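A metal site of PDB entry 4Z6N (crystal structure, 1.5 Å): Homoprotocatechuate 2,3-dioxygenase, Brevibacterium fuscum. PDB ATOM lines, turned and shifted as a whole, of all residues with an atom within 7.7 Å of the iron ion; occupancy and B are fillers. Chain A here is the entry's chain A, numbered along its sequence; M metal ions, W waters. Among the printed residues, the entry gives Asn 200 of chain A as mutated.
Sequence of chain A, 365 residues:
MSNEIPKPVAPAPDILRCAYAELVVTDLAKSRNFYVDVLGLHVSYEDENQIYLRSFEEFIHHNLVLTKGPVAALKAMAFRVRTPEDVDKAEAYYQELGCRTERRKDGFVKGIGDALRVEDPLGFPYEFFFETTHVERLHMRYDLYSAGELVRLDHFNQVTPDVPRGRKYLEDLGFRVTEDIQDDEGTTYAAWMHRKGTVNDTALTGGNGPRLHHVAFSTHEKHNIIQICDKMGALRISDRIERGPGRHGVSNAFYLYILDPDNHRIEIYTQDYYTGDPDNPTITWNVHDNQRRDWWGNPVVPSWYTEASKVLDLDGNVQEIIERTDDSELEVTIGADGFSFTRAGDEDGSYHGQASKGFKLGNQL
OE2 of Glu 267 sits at hydrogen-bond distance from OH of Tyr 257, at 3.3 Å.
The side-chain carboxylate of Glu 267 lies within hydrogen-bond range of a ring nitrogen (NE2) of His 248 (2.8 Å).
N of Glu 267 sits at hydrogen-bond distance from O of Val 215 (2.9 Å).
The backbone carbonyl oxygen of His 155 sits at hydrogen-bond distance from the backbone NH of Ala 216, at 2.8 Å.
The side-chain amide oxygen (OD1) of Asn 200 is in hydrogen-bond range of a ring nitrogen (ND1) of His 155 (3.3 Å).
ND1 of His 155 sits at hydrogen-bond distance from OD2 of Asp 154, at 2.7 Å.
The backbone carbonyl oxygen of His 214 lies within hydrogen-bond range of the backbone NH of Asn 157, at 3.0 Å.
A ring nitrogen (ND1) of His 214 is in hydrogen-bond range of a ring nitrogen (ND1) of His 213 (2.9 Å).
Of the 22 residues printed, 3 come within 4 Å of the iron ion.
The iron ion is bound by the side-chain carboxylate (OE1) of Glu 267, at 2.1 Å.
The iron ion is bound by water W3, 2.2 Å away.
The iron ion is bound by water W1 (2.2 Å).
NE2 of His 155 is bound to the iron ion.
A ring nitrogen (NE2) of His 214 is bound to the iron ion, 2.2 Å away.
Water W2 is bound to the iron ion, 2.3 Å away.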
ATOM      1  N   ASP A 154      18.390 -14.638  15.899  1.00  0.00           N
ATOM      2  CA  ASP A 154      18.120 -15.881  15.176  1.00  0.00           C
ATOM      3  C   ASP A 154      16.978 -16.725  15.764  1.00  0.00           C
ATOM      4  O   ASP A 154      16.104 -17.173  15.003  1.00  0.00           O
ATOM      5  CB  ASP A 154      19.354 -16.745  14.967  1.00  0.00           C
ATOM      6  CG  ASP A 154      19.071 -17.894  13.971  1.00  0.00           C
ATOM      7  OD1 ASP A 154      18.965 -17.609  12.743  1.00  0.00           O
ATOM      8  OD2 ASP A 154      18.842 -19.045  14.413  1.00  0.00           O
ATOM      9  N   HIS A 155      17.026 -16.995  17.066  1.00  0.00           N
ATOM     10  CA  HIS A 155      16.053 -17.898  17.685  1.00  0.00           C
ATOM     11  C   HIS A 155      15.996 -17.856  19.170  1.00  0.00           C
ATOM     12  O   HIS A 155      16.828 -17.288  19.821  1.00  0.00           O
ATOM     13  CB  HIS A 155      16.289 -19.368  17.236  1.00  0.00           C
ATOM     14  CG  HIS A 155      17.562 -19.971  17.725  1.00  0.00           C
ATOM     15  ND1 HIS A 155      18.704 -19.975  16.957  1.00  0.00           N
ATOM     16  CD2 HIS A 155      17.864 -20.650  18.855  1.00  0.00           C
ATOM     17  CE1 HIS A 155      19.673 -20.610  17.622  1.00  0.00           C
ATOM     18  NE2 HIS A 155      19.181 -21.034  18.761  1.00  0.00           N
ATOM     19  N   PHE A 156      14.979 -18.529  19.699  1.00  0.00           N
ATOM     20  CA  PHE A 156      14.852 -18.788  21.098  1.00  0.00           C
ATOM     21  C   PHE A 156      14.946 -20.314  21.310  1.00  0.00           C
ATOM     22  O   PHE A 156      14.752 -21.086  20.366  1.00  0.00           O
ATOM     23  CB  PHE A 156      13.453 -18.393  21.618  1.00  0.00           C
ATOM     24  CG  PHE A 156      12.987 -16.984  21.232  1.00  0.00           C
ATOM     25  CD1 PHE A 156      13.761 -15.869  21.513  1.00  0.00           C
ATOM     26  CD2 PHE A 156      11.762 -16.793  20.602  1.00  0.00           C
ATOM     27  CE1 PHE A 156      13.313 -14.606  21.181  1.00  0.00           C
ATOM     28  CE2 PHE A 156      11.317 -15.532  20.284  1.00  0.00           C
ATOM     29  CZ  PHE A 156      12.091 -14.445  20.548  1.00  0.00           C
ATOM     30  N   ASN A 157      15.234 -20.711  22.531  1.00  0.00           N
ATOM     31  CA  ASN A 157      15.199 -22.132  22.933  1.00  0.00           C
ATOM     32  C   ASN A 157      14.582 -22.245  24.325  1.00  0.00           C
ATOM     33  O   ASN A 157      15.038 -21.630  25.268  1.00  0.00           O
ATOM     34  CB  ASN A 157      16.623 -22.732  22.863  1.00  0.00           C
ATOM     35  CG  ASN A 157      16.643 -24.223  23.061  1.00  0.00           C
ATOM     36  OD1 ASN A 157      16.163 -24.700  24.066  1.00  0.00           O
ATOM     37  ND2 ASN A 157      17.213 -24.959  22.109  1.00  0.00           N
ATOM     38  N   TRP A 192      13.656 -28.778  17.120  1.00  0.00           N
ATOM     39  CA  TRP A 192      13.871 -27.461  16.559  1.00  0.00           C
ATOM     40  C   TRP A 192      12.852 -27.208  15.510  1.00  0.00           C
ATOM     41  O   TRP A 192      12.588 -28.073  14.684  1.00  0.00           O
ATOM     42  CB  TRP A 192      15.280 -27.389  15.966  1.00  0.00           C
ATOM     43  CG  TRP A 192      16.393 -27.323  16.965  1.00  0.00           C
ATOM     44  CD1 TRP A 192      17.131 -26.209  17.307  1.00  0.00           C
ATOM     45  CD2 TRP A 192      16.951 -28.406  17.727  1.00  0.00           C
ATOM     46  NE1 TRP A 192      18.066 -26.528  18.246  1.00  0.00           N
ATOM     47  CE2 TRP A 192      18.009 -27.873  18.508  1.00  0.00           C
ATOM     48  CE3 TRP A 192      16.685 -29.798  17.795  1.00  0.00           C
ATOM     49  CZ2 TRP A 192      18.775 -28.655  19.378  1.00  0.00           C
ATOM     50  CZ3 TRP A 192      17.441 -30.583  18.682  1.00  0.00           C
ATOM     51  CH2 TRP A 192      18.473 -30.012  19.466  1.00  0.00           C
ATOM     52  N   ASN A 200      15.786 -22.862  13.042  1.00  0.00           N
ATOM     53  CA  ASN A 200      14.769 -22.551  14.036  1.00  0.00           C
ATOM     54  C   ASN A 200      14.419 -21.093  14.248  1.00  0.00           C
ATOM     55  O   ASN A 200      15.221 -20.188  14.047  1.00  0.00           O
ATOM     56  CB  ASN A 200      14.985 -23.301  15.350  1.00  0.00           C
ATOM     57  CG  ASN A 200      16.198 -22.871  16.111  1.00  0.00           C
ATOM     58  OD1 ASN A 200      17.253 -22.532  15.531  1.00  0.00           O
ATOM     59  ND2 ASN A 200      16.069 -22.912  17.466  1.00  0.00           N
ATOM     60  N   ALA A 203      12.717 -23.490  19.764  1.00  0.00           N
ATOM     61  CA  ALA A 203      13.102 -24.863  19.954  1.00  0.00           C
ATOM     62  C   ALA A 203      12.727 -25.304  21.325  1.00  0.00           C
ATOM     63  O   ALA A 203      12.493 -24.500  22.242  1.00  0.00           O
ATOM     64  CB  ALA A 203      14.608 -25.020  19.731  1.00  0.00           C
ATOM     65  N   THR A 205      13.831 -27.908  24.471  1.00  0.00           N
ATOM     66  CA  THR A 205      14.800 -28.766  25.143  1.00  0.00           C
ATOM     67  C   THR A 205      14.093 -29.416  26.299  1.00  0.00           C
ATOM     68  O   THR A 205      13.459 -28.730  27.108  1.00  0.00           O
ATOM     69  CB  THR A 205      15.998 -27.933  25.662  1.00  0.00           C
ATOM     70  OG1 THR A 205      16.611 -27.267  24.546  1.00  0.00           O
ATOM     71  CG2 THR A 205      17.009 -28.801  26.440  1.00  0.00           C
ATOM     72  N   HIS A 213      15.834 -21.517  27.833  1.00  0.00           N
ATOM     73  CA  HIS A 213      17.184 -21.957  27.724  1.00  0.00           C
ATOM     74  C   HIS A 213      18.141 -20.888  27.220  1.00  0.00           C
ATOM     75  O   HIS A 213      19.168 -20.645  27.870  1.00  0.00           O
ATOM     76  CB  HIS A 213      17.290 -23.219  26.882  1.00  0.00           C
ATOM     77  CG  HIS A 213      18.561 -23.974  27.128  1.00  0.00           C
ATOM     78  ND1 HIS A 213      19.757 -23.576  26.585  1.00  0.00           N
ATOM     79  CD2 HIS A 213      18.862 -24.983  27.984  1.00  0.00           C
ATOM     80  CE1 HIS A 213      20.722 -24.353  27.009  1.00  0.00           C
ATOM     81  NE2 HIS A 213      20.204 -25.220  27.861  1.00  0.00           N
ATOM     82  N   HIS A 214      17.861 -20.302  26.038  1.00  0.00           N
ATOM     83  CA  HIS A 214      18.716 -19.228  25.569  1.00  0.00           C
ATOM     84  C   HIS A 214      18.004 -18.388  24.529  1.00  0.00           C
ATOM     85  O   HIS A 214      16.977 -18.799  24.002  1.00  0.00           O
ATOM     86  CB  HIS A 214      20.051 -19.762  24.985  1.00  0.00           C
ATOM     87  CG  HIS A 214      19.897 -20.771  23.868  1.00  0.00           C
ATOM     88  ND1 HIS A 214      19.896 -22.119  24.115  1.00  0.00           N
ATOM     89  CD2 HIS A 214      19.827 -20.631  22.529  1.00  0.00           C
ATOM     90  CE1 HIS A 214      19.817 -22.784  22.976  1.00  0.00           C
ATOM     91  NE2 HIS A 214      19.773 -21.906  21.990  1.00  0.00           N
ATOM     92  N   VAL A 215      18.629 -17.228  24.244  1.00  0.00           N
ATOM     93  CA  VAL A 215      18.335 -16.424  23.094  1.00  0.00           C
ATOM     94  C   VAL A 215      19.558 -16.454  22.193  1.00  0.00           C
ATOM     95  O   VAL A 215      20.650 -16.349  22.703  1.00  0.00           O
ATOM     96  CB  VAL A 215      17.972 -14.964  23.523  1.00  0.00           C
ATOM     97  CG1 VAL A 215      17.660 -14.144  22.306  1.00  0.00           C
ATOM     98  CG2 VAL A 215      16.745 -14.992  24.470  1.00  0.00           C
ATOM     99  N   ALA A 216      19.368 -16.601  20.871  1.00  0.00           N
ATOM    100  CA  ALA A 216      20.510 -16.730  19.974  1.00  0.00           C
ATOM    101  C   ALA A 216      20.562 -15.531  19.010  1.00  0.00           C
ATOM    102  O   ALA A 216      19.534 -15.192  18.397  1.00  0.00           O
ATOM    103  CB  ALA A 216      20.426 -18.026  19.177  1.00  0.00           C
ATOM    104  N   HIS A 248      27.884 -27.211  15.761  1.00  0.00           N
ATOM    105  CA  HIS A 248      26.770 -28.065  16.128  1.00  0.00           C
ATOM    106  C   HIS A 248      26.633 -29.255  15.164  1.00  0.00           C
ATOM    107  O   HIS A 248      26.884 -29.121  13.970  1.00  0.00           O
ATOM    108  CB  HIS A 248      25.434 -27.296  16.046  1.00  0.00           C
ATOM    109  CG  HIS A 248      25.146 -26.439  17.224  1.00  0.00           C
ATOM    110  ND1 HIS A 248      25.220 -26.899  18.530  1.00  0.00           N
ATOM    111  CD2 HIS A 248      24.751 -25.152  17.306  1.00  0.00           C
ATOM    112  CE1 HIS A 248      24.875 -25.922  19.353  1.00  0.00           C
ATOM    113  NE2 HIS A 248      24.580 -24.859  18.640  1.00  0.00           N
ATOM    114  N   VAL A 250      23.258 -30.927  15.262  1.00  0.00           N
ATOM    115  CA  VAL A 250      21.955 -30.311  15.054  1.00  0.00           C
ATOM    116  C   VAL A 250      22.115 -28.851  14.675  1.00  0.00           C
ATOM    117  O   VAL A 250      22.666 -28.083  15.455  1.00  0.00           O
ATOM    118  CB  VAL A 250      21.072 -30.355  16.323  1.00  0.00           C
ATOM    119  CG1 VAL A 250      19.795 -29.578  16.065  1.00  0.00           C
ATOM    120  CG2 VAL A 250      20.724 -31.783  16.701  1.00  0.00           C
ATOM    121  N   SER A 251      21.654 -28.531  13.454  1.00  0.00           N
ATOM    122  CA  SER A 251      21.669 -27.196  12.835  1.00  0.00           C
ATOM    123  C   SER A 251      22.901 -26.946  11.968  1.00  0.00           C
ATOM    124  O   SER A 251      22.854 -26.093  11.105  1.00  0.00           O
ATOM    125  CB  SER A 251      21.531 -26.041  13.851  1.00  0.00           C
ATOM    126  OG  SER A 251      22.794 -25.705  14.435  1.00  0.00           O
ATOM    127  N   TYR A 255      28.899 -22.145  16.786  1.00  0.00           N
ATOM    128  CA  TYR A 255      28.219 -21.651  17.968  1.00  0.00           C
ATOM    129  C   TYR A 255      29.104 -21.366  19.143  1.00  0.00           C
ATOM    130  O   TYR A 255      30.263 -21.807  19.214  1.00  0.00           O
ATOM    131  CB  TYR A 255      27.126 -22.667  18.424  1.00  0.00           C
ATOM    132  CG  TYR A 255      27.701 -23.882  19.124  1.00  0.00           C
ATOM    133  CD1 TYR A 255      28.072 -25.018  18.381  1.00  0.00           C
ATOM    134  CD2 TYR A 255      27.960 -23.873  20.473  1.00  0.00           C
ATOM    135  CE1 TYR A 255      28.647 -26.125  19.018  1.00  0.00           C
ATOM    136  CE2 TYR A 255      28.542 -24.960  21.118  1.00  0.00           C
ATOM    137  CZ  TYR A 255      28.876 -26.090  20.378  1.00  0.00           C
ATOM    138  OH  TYR A 255      29.442 -27.202  20.974  1.00  0.00           O
ATOM    139  N   TYR A 257      28.125 -20.431  23.605  1.00  0.00           N
ATOM    140  CA  TYR A 257      27.180 -20.081  24.672  1.00  0.00           C
ATOM    141  C   TYR A 257      27.924 -19.327  25.789  1.00  0.00           C
ATOM    142  O   TYR A 257      28.924 -19.815  26.359  1.00  0.00           O
ATOM    143  CB  TYR A 257      26.544 -21.334  25.287  1.00  0.00           C
ATOM    144  CG  TYR A 257      25.739 -22.165  24.332  1.00  0.00           C
ATOM    145  CD1 TYR A 257      24.412 -21.855  24.041  1.00  0.00           C
ATOM    146  CD2 TYR A 257      26.295 -23.268  23.706  1.00  0.00           C
ATOM    147  CE1 TYR A 257      23.681 -22.604  23.133  1.00  0.00           C
ATOM    148  CE2 TYR A 257      25.555 -24.016  22.794  1.00  0.00           C
ATOM    149  CZ  TYR A 257      24.247 -23.697  22.528  1.00  0.00           C
ATOM    150  OH  TYR A 257      23.510 -24.422  21.668  1.00  0.00           O
ATOM    151  N   GLU A 267      23.248 -17.533  23.053  1.00  0.00           N
ATOM    152  CA  GLU A 267      24.015 -18.240  22.025  1.00  0.00           C
ATOM    153  C   GLU A 267      24.432 -17.272  20.931  1.00  0.00           C
ATOM    154  O   GLU A 267      23.663 -16.409  20.545  1.00  0.00           O
ATOM    155  CB  GLU A 267      23.163 -19.343  21.428  1.00  0.00           C
ATOM    156  CG  GLU A 267      23.932 -20.240  20.461  1.00  0.00           C
ATOM    157  CD  GLU A 267      23.106 -21.320  19.860  1.00  0.00           C
ATOM    158  OE1 GLU A 267      21.894 -21.314  20.066  1.00  0.00           O
ATOM    159  OE2 GLU A 267      23.672 -22.228  19.229  1.00  0.00           O
ATOM    160  N   ILE A 268      25.665 -17.431  20.425  1.00  0.00           N
ATOM    161  CA  ILE A 268      26.080 -16.783  19.211  1.00  0.00           C
ATOM    162  C   ILE A 268      26.198 -17.886  18.170  1.00  0.00           C
ATOM    163  O   ILE A 268      26.656 -19.012  18.461  1.00  0.00           O
ATOM    164  CB  ILE A 268      27.420 -16.044  19.384  1.00  0.00           C
ATOM    165  CG1 ILE A 268      27.596 -15.412  20.788  1.00  0.00           C
ATOM    166  CG2 ILE A 268      27.577 -15.044  18.235  1.00  0.00           C
ATOM    167  CD1 ILE A 268      26.652 -14.298  21.088  1.00  0.00           C
ATOM    168  N   TYR A 269      25.760 -17.587  16.969  1.00  0.00           N
ATOM    169  CA  TYR A 269      25.381 -18.637  15.993  1.00  0.00           C
ATOM    170  C   TYR A 269      25.670 -18.159  14.590  1.00  0.00           C
ATOM    171  O   TYR A 269      25.424 -17.010  14.276  1.00  0.00           O
ATOM    172  CB  TYR A 269      23.883 -18.861  16.198  1.00  0.00           C
ATOM    173  CG  TYR A 269      23.118 -19.938  15.457  1.00  0.00           C
ATOM    174  CD1 TYR A 269      22.959 -21.216  16.000  1.00  0.00           C
ATOM    175  CD2 TYR A 269      22.472 -19.638  14.251  1.00  0.00           C
ATOM    176  CE1 TYR A 269      22.144 -22.150  15.374  1.00  0.00           C
ATOM    177  CE2 TYR A 269      21.696 -20.575  13.600  1.00  0.00           C
ATOM    178  CZ  TYR A 269      21.525 -21.837  14.162  1.00  0.00           C
ATOM    179  OH  TYR A 269      20.722 -22.772  13.555  1.00  0.00           O
ATOM    180  N   ARG A 293      25.449 -32.735  19.303  1.00  0.00           N
ATOM    181  CA  ARG A 293      25.395 -31.395  19.884  1.00  0.00           C
ATOM    182  C   ARG A 293      26.620 -30.591  19.528  1.00  0.00           C
ATOM    183  O   ARG A 293      26.508 -29.480  19.051  1.00  0.00           O
ATOM    184  CB  ARG A 293      25.173 -31.454  21.393  1.00  0.00           C
ATOM    185  CG  ARG A 293      23.739 -31.883  21.752  1.00  0.00           C
ATOM    186  CD  ARG A 293      23.279 -31.378  23.092  1.00  0.00           C
ATOM    187  NE  ARG A 293      21.846 -31.614  23.286  1.00  0.00           N
ATOM    188  CZ  ARG A 293      20.832 -30.821  22.942  1.00  0.00           C
ATOM    189  NH1 ARG A 293      21.007 -29.675  22.337  1.00  0.00           N
ATOM    190  NH2 ARG A 293      19.589 -31.198  23.272  1.00  0.00           N
ATOM    191  N   TRP A 304      24.897 -26.778  31.159  1.00  0.00           N
ATOM    192  CA  TRP A 304      24.132 -26.489  29.938  1.00  0.00           C
ATOM    193  C   TRP A 304      22.781 -27.194  29.977  1.00  0.00           C
ATOM    194  O   TRP A 304      21.754 -26.693  29.453  1.00  0.00           O
ATOM    195  CB  TRP A 304      24.970 -26.866  28.683  1.00  0.00           C
ATOM    196  CG  TRP A 304      24.414 -26.287  27.417  1.00  0.00           C
ATOM    197  CD1 TRP A 304      24.725 -25.093  26.856  1.00  0.00           C
ATOM    198  CD2 TRP A 304      23.420 -26.877  26.570  1.00  0.00           C
ATOM    199  NE1 TRP A 304      24.000 -24.881  25.727  1.00  0.00           N
ATOM    200  CE2 TRP A 304      23.201 -25.976  25.506  1.00  0.00           C
ATOM    201  CE3 TRP A 304      22.703 -28.076  26.603  1.00  0.00           C
ATOM    202  CZ2 TRP A 304      22.266 -26.217  24.510  1.00  0.00           C
ATOM    203  CZ3 TRP A 304      21.794 -28.317  25.623  1.00  0.00           C
ATOM    204  CH2 TRP A 304      21.583 -27.387  24.581  1.00  0.00           C
HETATM  205 FE    FE M   1      20.208 -22.569  19.944  1.00  0.00          FE
HETATM  206  O   HOH W   1      21.181 -23.439  18.195  1.00  0.00           O
HETATM  207  O   HOH W   2      21.182 -24.458  20.842  1.00  0.00           O
HETATM  208  O   HOH W   3      18.424 -23.777  19.772  1.00  0.00           O
